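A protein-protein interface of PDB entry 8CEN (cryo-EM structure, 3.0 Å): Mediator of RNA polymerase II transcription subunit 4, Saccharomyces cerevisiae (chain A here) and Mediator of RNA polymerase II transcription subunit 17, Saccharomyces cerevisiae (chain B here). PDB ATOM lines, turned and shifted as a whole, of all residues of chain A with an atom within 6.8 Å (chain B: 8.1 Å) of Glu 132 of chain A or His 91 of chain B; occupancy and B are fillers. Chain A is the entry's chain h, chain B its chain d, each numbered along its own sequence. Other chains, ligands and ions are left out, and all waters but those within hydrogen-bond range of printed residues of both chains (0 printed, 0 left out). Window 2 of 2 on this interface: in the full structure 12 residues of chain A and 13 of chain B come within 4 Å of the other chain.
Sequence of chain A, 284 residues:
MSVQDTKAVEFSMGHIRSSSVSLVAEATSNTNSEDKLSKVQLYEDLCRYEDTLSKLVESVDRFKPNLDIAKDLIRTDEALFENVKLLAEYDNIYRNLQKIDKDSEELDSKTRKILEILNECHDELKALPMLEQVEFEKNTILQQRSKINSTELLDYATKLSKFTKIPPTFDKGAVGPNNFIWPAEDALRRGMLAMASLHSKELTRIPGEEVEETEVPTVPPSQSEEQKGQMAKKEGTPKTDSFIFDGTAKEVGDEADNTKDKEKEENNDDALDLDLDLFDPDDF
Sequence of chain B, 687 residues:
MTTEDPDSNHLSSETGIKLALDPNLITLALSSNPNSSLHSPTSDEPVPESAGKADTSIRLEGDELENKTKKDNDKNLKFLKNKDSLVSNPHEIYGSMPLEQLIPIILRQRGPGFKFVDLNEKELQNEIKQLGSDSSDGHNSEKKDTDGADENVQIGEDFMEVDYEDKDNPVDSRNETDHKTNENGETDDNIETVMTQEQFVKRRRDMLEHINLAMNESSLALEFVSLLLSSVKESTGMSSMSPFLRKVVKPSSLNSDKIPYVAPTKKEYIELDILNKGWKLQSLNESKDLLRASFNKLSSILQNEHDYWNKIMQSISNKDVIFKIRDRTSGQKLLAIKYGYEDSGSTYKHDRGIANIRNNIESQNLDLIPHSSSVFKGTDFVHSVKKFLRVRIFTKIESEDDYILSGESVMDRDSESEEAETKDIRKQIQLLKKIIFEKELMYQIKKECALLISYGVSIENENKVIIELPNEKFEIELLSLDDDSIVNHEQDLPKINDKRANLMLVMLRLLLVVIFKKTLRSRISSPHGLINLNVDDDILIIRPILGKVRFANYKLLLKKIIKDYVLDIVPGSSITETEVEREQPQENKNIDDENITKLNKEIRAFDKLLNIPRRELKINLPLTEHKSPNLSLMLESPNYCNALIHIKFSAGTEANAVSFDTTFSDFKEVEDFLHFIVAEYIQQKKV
The side-chain carboxylate (OE1) of Glu 132 of chain A lies within hydrogen-bond range of a ring nitrogen (NE2) of His 91 of chain B, at 3.2 Å.
The backbone NH (N) of His 91 of chain B sits close to the side-chain amide oxygen (OD1) of Asn 89 of chain B (3.5 Å). The backbone carbonyl oxygen (O) of Glu 92 of chain B is in hydrogen-bond range of the side-chain hydroxyl (OG) of Ser 96 of chain B (3.2 Å). The backbone NH of Met 130 of chain A lies within hydrogen-bond range of the side-chain amide oxygen of Gln 133 of chain A (3.2 Å).
Asn 89 of chain B touches Gln 133 of chain A. Gln 133 of chain A touches His 91 of chain B. CB of Glu 92 of chain B touches NE2 of Gln 133 of chain A, at 3.8 Å. CD2 of Phe 136 of chain A touches OD1 of Asn 89 of chain B, at 3.2 Å. CD of Pro 90 of chain B touches CE2 of Phe 136 of chain A, 3.97 Å away. Glu 137 of chain A touches Asn 89 of chain B (CG to ND2, 3.99 Å).
Glu 132 of chain A touches just one residue of chain B: His 91 (3.2 Å). Printed residues of chain B within 4 Å of Phe 136 of chain A: Asn 89 (3.2 Å) and Pro 90 (3.97 Å). Of the printed residues of chain B, Glu 137 of chain A touches Asn 89. Of the printed residues of chain A, Pro 90 of chain B touches Phe 136. Of the printed residues of chain A, His 91 of chain B touches Glu 132 and Gln 133. Ser 96 of chain B touches none of the printed residues of chain A. Met 97 of chain B touches none of the printed residues of chain A. The nearest residue of chain A that does not touch His 91 of chain B is Met 130 of chain A (5.1 Å). The nearest printed residue of chain B that does not touch Gln 133 of chain A is Gly 95 of chain B (6.0 Å).
Hydrophobic or aromatic side chains of chain B that line the printed part of chain A: Pro 90 and His 91. Hydrophobic or aromatic side chains of chain A within 4 Å of the printed part of chain B: Phe 136. Among the printed residues, no Asp or Glu carboxylate lies within 4 Å of a Lys or Arg side-chain nitrogen of the other chain.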
ATOM      1  N   PRO A 129       5.841 -28.494 -32.934  1.00  0.00           N
ATOM      2  CA  PRO A 129       5.572 -28.927 -31.554  1.00  0.00           C
ATOM      3  C   PRO A 129       6.275 -30.230 -31.198  1.00  0.00           C
ATOM      4  O   PRO A 129       6.537 -31.075 -32.055  1.00  0.00           O
ATOM      5  CB  PRO A 129       4.050 -29.097 -31.530  1.00  0.00           C
ATOM      6  CG  PRO A 129       3.562 -28.150 -32.560  1.00  0.00           C
ATOM      7  CD  PRO A 129       4.592 -28.174 -33.652  1.00  0.00           C
ATOM      8  N   MET A 130       6.567 -30.391 -29.910  1.00  0.00           N
ATOM      9  CA  MET A 130       7.405 -31.480 -29.432  1.00  0.00           C
ATOM     10  C   MET A 130       6.574 -32.689 -28.997  1.00  0.00           C
ATOM     11  O   MET A 130       5.343 -32.640 -28.897  1.00  0.00           O
ATOM     12  CB  MET A 130       8.287 -31.001 -28.278  1.00  0.00           C
ATOM     13  CG  MET A 130       9.328 -29.972 -28.686  1.00  0.00           C
ATOM     14  SD  MET A 130      10.296 -29.367 -27.294  1.00  0.00           S
ATOM     15  CE  MET A 130      11.277 -30.816 -26.915  1.00  0.00           C
ATOM     16  N   LEU A 131       7.285 -33.789 -28.725  1.00  0.00           N
ATOM     17  CA  LEU A 131       6.636 -35.066 -28.437  1.00  0.00           C
ATOM     18  C   LEU A 131       5.928 -35.044 -27.089  1.00  0.00           C
ATOM     19  O   LEU A 131       4.786 -35.501 -26.972  1.00  0.00           O
ATOM     20  CB  LEU A 131       7.659 -36.199 -28.490  1.00  0.00           C
ATOM     21  CG  LEU A 131       7.117 -37.587 -28.146  1.00  0.00           C
ATOM     22  CD1 LEU A 131       6.198 -38.082 -29.248  1.00  0.00           C
ATOM     23  CD2 LEU A 131       8.253 -38.568 -27.910  1.00  0.00           C
ATOM     24  N   GLU A 132       6.590 -34.519 -26.056  1.00  0.00           N
ATOM     25  CA  GLU A 132       5.935 -34.413 -24.758  1.00  0.00           C
ATOM     26  C   GLU A 132       4.781 -33.418 -24.809  1.00  0.00           C
ATOM     27  O   GLU A 132       3.775 -33.602 -24.117  1.00  0.00           O
ATOM     28  CB  GLU A 132       6.957 -34.030 -23.685  1.00  0.00           C
ATOM     29  CG  GLU A 132       6.405 -33.970 -22.269  1.00  0.00           C
ATOM     30  CD  GLU A 132       7.469 -33.640 -21.240  1.00  0.00           C
ATOM     31  OE1 GLU A 132       8.636 -33.436 -21.635  1.00  0.00           O
ATOM     32  OE2 GLU A 132       7.139 -33.588 -20.037  1.00  0.00           O
ATOM     33  N   GLN A 133       4.884 -32.403 -25.672  1.00  0.00           N
ATOM     34  CA  GLN A 133       3.793 -31.451 -25.853  1.00  0.00           C
ATOM     35  C   GLN A 133       2.561 -32.121 -26.454  1.00  0.00           C
ATOM     36  O   GLN A 133       1.440 -31.939 -25.964  1.00  0.00           O
ATOM     37  CB  GLN A 133       4.258 -30.294 -26.737  1.00  0.00           C
ATOM     38  CG  GLN A 133       3.198 -29.242 -26.992  1.00  0.00           C
ATOM     39  CD  GLN A 133       3.607 -28.263 -28.071  1.00  0.00           C
ATOM     40  OE1 GLN A 133       4.787 -28.142 -28.397  1.00  0.00           O
ATOM     41  NE2 GLN A 133       2.631 -27.559 -28.633  1.00  0.00           N
ATOM     42  N   VAL A 134       2.747 -32.910 -27.517  1.00  0.00           N
ATOM     43  CA  VAL A 134       1.580 -33.537 -28.134  1.00  0.00           C
ATOM     44  C   VAL A 134       1.045 -34.673 -27.267  1.00  0.00           C
ATOM     45  O   VAL A 134      -0.163 -34.943 -27.272  1.00  0.00           O
ATOM     46  CB  VAL A 134       1.885 -34.000 -29.573  1.00  0.00           C
ATOM     47  CG1 VAL A 134       2.119 -32.798 -30.475  1.00  0.00           C
ATOM     48  CG2 VAL A 134       3.069 -34.932 -29.615  1.00  0.00           C
ATOM     49  N   GLU A 135       1.905 -35.332 -26.480  1.00  0.00           N
ATOM     50  CA  GLU A 135       1.399 -36.319 -25.526  1.00  0.00           C
ATOM     51  C   GLU A 135       0.606 -35.658 -24.406  1.00  0.00           C
ATOM     52  O   GLU A 135      -0.393 -36.216 -23.939  1.00  0.00           O
ATOM     53  CB  GLU A 135       2.543 -37.159 -24.954  1.00  0.00           C
ATOM     54  CG  GLU A 135       3.234 -38.105 -25.942  1.00  0.00           C
ATOM     55  CD  GLU A 135       2.484 -39.411 -26.195  1.00  0.00           C
ATOM     56  OE1 GLU A 135       1.234 -39.437 -26.160  1.00  0.00           O
ATOM     57  OE2 GLU A 135       3.163 -40.432 -26.428  1.00  0.00           O
ATOM     58  N   PHE A 136       1.025 -34.469 -23.962  1.00  0.00           N
ATOM     59  CA  PHE A 136       0.247 -33.748 -22.960  1.00  0.00           C
ATOM     60  C   PHE A 136      -1.084 -33.273 -23.533  1.00  0.00           C
ATOM     61  O   PHE A 136      -2.100 -33.274 -22.830  1.00  0.00           O
ATOM     62  CB  PHE A 136       1.047 -32.569 -22.409  1.00  0.00           C
ATOM     63  CG  PHE A 136       0.414 -31.919 -21.212  1.00  0.00           C
ATOM     64  CD1 PHE A 136       0.493 -32.513 -19.963  1.00  0.00           C
ATOM     65  CD2 PHE A 136      -0.264 -30.717 -21.334  1.00  0.00           C
ATOM     66  CE1 PHE A 136      -0.089 -31.920 -18.858  1.00  0.00           C
ATOM     67  CE2 PHE A 136      -0.849 -30.118 -20.233  1.00  0.00           C
ATOM     68  CZ  PHE A 136      -0.761 -30.721 -18.994  1.00  0.00           C
ATOM     69  N   GLU A 137      -1.096 -32.872 -24.809  1.00  0.00           N
ATOM     70  CA  GLU A 137      -2.360 -32.533 -25.463  1.00  0.00           C
ATOM     71  C   GLU A 137      -3.283 -33.744 -25.555  1.00  0.00           C
ATOM     72  O   GLU A 137      -4.493 -33.628 -25.322  1.00  0.00           O
ATOM     73  CB  GLU A 137      -2.106 -31.955 -26.856  1.00  0.00           C
ATOM     74  CG  GLU A 137      -1.416 -30.602 -26.868  1.00  0.00           C
ATOM     75  CD  GLU A 137      -1.176 -30.090 -28.276  1.00  0.00           C
ATOM     76  OE1 GLU A 137      -1.436 -30.845 -29.235  1.00  0.00           O
ATOM     77  OE2 GLU A 137      -0.731 -28.933 -28.424  1.00  0.00           O
ATOM     78  N   ASN A 139      -3.246 -36.367 -23.538  1.00  0.00           N
ATOM     79  CA  ASN A 139      -3.694 -36.650 -22.179  1.00  0.00           C
ATOM     80  C   ASN A 139      -4.785 -35.681 -21.741  1.00  0.00           C
ATOM     81  O   ASN A 139      -5.737 -36.080 -21.065  1.00  0.00           O
ATOM     82  CB  ASN A 139      -2.511 -36.602 -21.214  1.00  0.00           C
ATOM     83  CG  ASN A 139      -1.554 -37.760 -21.410  1.00  0.00           C
ATOM     84  OD1 ASN A 139      -1.973 -38.900 -21.610  1.00  0.00           O
ATOM     85  ND2 ASN A 139      -0.257 -37.473 -21.358  1.00  0.00           N
ATOM     86  N   SER B  88      -3.305 -24.819 -19.037  1.00  0.00           N
ATOM     87  CA  SER B  88      -1.940 -24.308 -19.147  1.00  0.00           C
ATOM     88  C   SER B  88      -1.021 -25.436 -19.595  1.00  0.00           C
ATOM     89  O   SER B  88      -0.561 -26.241 -18.783  1.00  0.00           O
ATOM     90  CB  SER B  88      -1.483 -23.716 -17.819  1.00  0.00           C
ATOM     91  OG  SER B  88      -1.420 -24.710 -16.812  1.00  0.00           O
ATOM     92  N   ASN B  89      -0.753 -25.496 -20.894  1.00  0.00           N
ATOM     93  CA  ASN B  89       0.229 -26.434 -21.420  1.00  0.00           C
ATOM     94  C   ASN B  89       1.622 -25.850 -21.219  1.00  0.00           C
ATOM     95  O   ASN B  89       1.927 -24.798 -21.788  1.00  0.00           O
ATOM     96  CB  ASN B  89      -0.035 -26.697 -22.900  1.00  0.00           C
ATOM     97  CG  ASN B  89       0.829 -27.810 -23.471  1.00  0.00           C
ATOM     98  OD1 ASN B  89       1.547 -28.500 -22.748  1.00  0.00           O
ATOM     99  ND2 ASN B  89       0.759 -27.990 -24.785  1.00  0.00           N
ATOM    100  N   PRO B  90       2.489 -26.488 -20.424  1.00  0.00           N
ATOM    101  CA  PRO B  90       3.808 -25.896 -20.147  1.00  0.00           C
ATOM    102  C   PRO B  90       4.767 -25.918 -21.326  1.00  0.00           C
ATOM    103  O   PRO B  90       5.791 -25.226 -21.273  1.00  0.00           O
ATOM    104  CB  PRO B  90       4.338 -26.756 -18.992  1.00  0.00           C
ATOM    105  CG  PRO B  90       3.653 -28.066 -19.168  1.00  0.00           C
ATOM    106  CD  PRO B  90       2.274 -27.728 -19.660  1.00  0.00           C
ATOM    107  N   HIS B  91       4.483 -26.678 -22.381  1.00  0.00           N
ATOM    108  CA  HIS B  91       5.375 -26.735 -23.531  1.00  0.00           C
ATOM    109  C   HIS B  91       4.961 -25.808 -24.662  1.00  0.00           C
ATOM    110  O   HIS B  91       5.830 -25.288 -25.368  1.00  0.00           O
ATOM    111  CB  HIS B  91       5.466 -28.167 -24.065  1.00  0.00           C
ATOM    112  CG  HIS B  91       6.118 -29.127 -23.121  1.00  0.00           C
ATOM    113  ND1 HIS B  91       5.556 -29.486 -21.916  1.00  0.00           N
ATOM    114  CD2 HIS B  91       7.288 -29.803 -23.206  1.00  0.00           C
ATOM    115  CE1 HIS B  91       6.350 -30.343 -21.299  1.00  0.00           C
ATOM    116  NE2 HIS B  91       7.410 -30.550 -22.060  1.00  0.00           N
ATOM    117  N   GLU B  92       3.657 -25.584 -24.848  1.00  0.00           N
ATOM    118  CA  GLU B  92       3.194 -24.716 -25.925  1.00  0.00           C
ATOM    119  C   GLU B  92       3.560 -23.260 -25.663  1.00  0.00           C
ATOM    120  O   GLU B  92       3.779 -22.497 -26.611  1.00  0.00           O
ATOM    121  CB  GLU B  92       1.680 -24.889 -26.105  1.00  0.00           C
ATOM    122  CG  GLU B  92       1.056 -24.233 -27.344  1.00  0.00           C
ATOM    123  CD  GLU B  92       0.724 -22.762 -27.159  1.00  0.00           C
ATOM    124  OE1 GLU B  92       0.448 -22.351 -26.012  1.00  0.00           O
ATOM    125  OE2 GLU B  92       0.738 -22.019 -28.162  1.00  0.00           O
ATOM    126  N   ILE B  93       3.652 -22.861 -24.391  1.00  0.00           N
ATOM    127  CA  ILE B  93       3.961 -21.475 -24.052  1.00  0.00           C
ATOM    128  C   ILE B  93       5.454 -21.186 -24.002  1.00  0.00           C
ATOM    129  O   ILE B  93       5.842 -20.010 -23.940  1.00  0.00           O
ATOM    130  CB  ILE B  93       3.343 -21.086 -22.695  1.00  0.00           C
ATOM    131  CG1 ILE B  93       3.760 -22.089 -21.617  1.00  0.00           C
ATOM    132  CG2 ILE B  93       1.828 -21.002 -22.806  1.00  0.00           C
ATOM    133  CD1 ILE B  93       3.105 -21.858 -20.271  1.00  0.00           C
ATOM    134  N   TYR B  94       6.303 -22.209 -24.032  1.00  0.00           N
ATOM    135  CA  TYR B  94       7.736 -22.003 -23.860  1.00  0.00           C
ATOM    136  C   TYR B  94       8.574 -22.520 -25.018  1.00  0.00           C
ATOM    137  O   TYR B  94       9.555 -21.873 -25.393  1.00  0.00           O
ATOM    138  CB  TYR B  94       8.206 -22.665 -22.554  1.00  0.00           C
ATOM    139  CG  TYR B  94       7.731 -21.949 -21.308  1.00  0.00           C
ATOM    140  CD1 TYR B  94       7.754 -20.565 -21.229  1.00  0.00           C
ATOM    141  CD2 TYR B  94       7.255 -22.658 -20.214  1.00  0.00           C
ATOM    142  CE1 TYR B  94       7.319 -19.904 -20.097  1.00  0.00           C
ATOM    143  CE2 TYR B  94       6.812 -22.006 -19.078  1.00  0.00           C
ATOM    144  CZ  TYR B  94       6.850 -20.629 -19.025  1.00  0.00           C
ATOM    145  OH  TYR B  94       6.416 -19.974 -17.896  1.00  0.00           O
ATOM    146  N   GLY B  95       8.221 -23.672 -25.592  1.00  0.00           N
ATOM    147  CA  GLY B  95       9.035 -24.241 -26.654  1.00  0.00           C
ATOM    148  C   GLY B  95       8.973 -23.460 -27.953  1.00  0.00           C
ATOM    149  O   GLY B  95       9.969 -23.360 -28.675  1.00  0.00           O
ATOM    150  N   SER B  96       7.802 -22.902 -28.275  1.00  0.00           N
ATOM    151  CA  SER B  96       7.608 -22.283 -29.584  1.00  0.00           C
ATOM    152  C   SER B  96       8.340 -20.952 -29.712  1.00  0.00           C
ATOM    153  O   SER B  96       8.838 -20.628 -30.795  1.00  0.00           O
ATOM    154  CB  SER B  96       6.115 -22.089 -29.853  1.00  0.00           C
ATOM    155  OG  SER B  96       5.543 -21.189 -28.922  1.00  0.00           O
ATOM    156  N   MET B  97       8.413 -20.172 -28.638  1.00  0.00           N
ATOM    157  CA  MET B  97       8.989 -18.840 -28.716  1.00  0.00           C
ATOM    158  C   MET B  97      10.515 -18.914 -28.787  1.00  0.00           C
ATOM    159  O   MET B  97      11.112 -19.915 -28.385  1.00  0.00           O
ATOM    160  CB  MET B  97       8.545 -18.007 -27.514  1.00  0.00           C
ATOM    161  CG  MET B  97       9.052 -18.480 -26.170  1.00  0.00           C
ATOM    162  SD  MET B  97       8.393 -17.413 -24.877  1.00  0.00           S
ATOM    163  CE  MET B  97       9.104 -18.157 -23.421  1.00  0.00           C
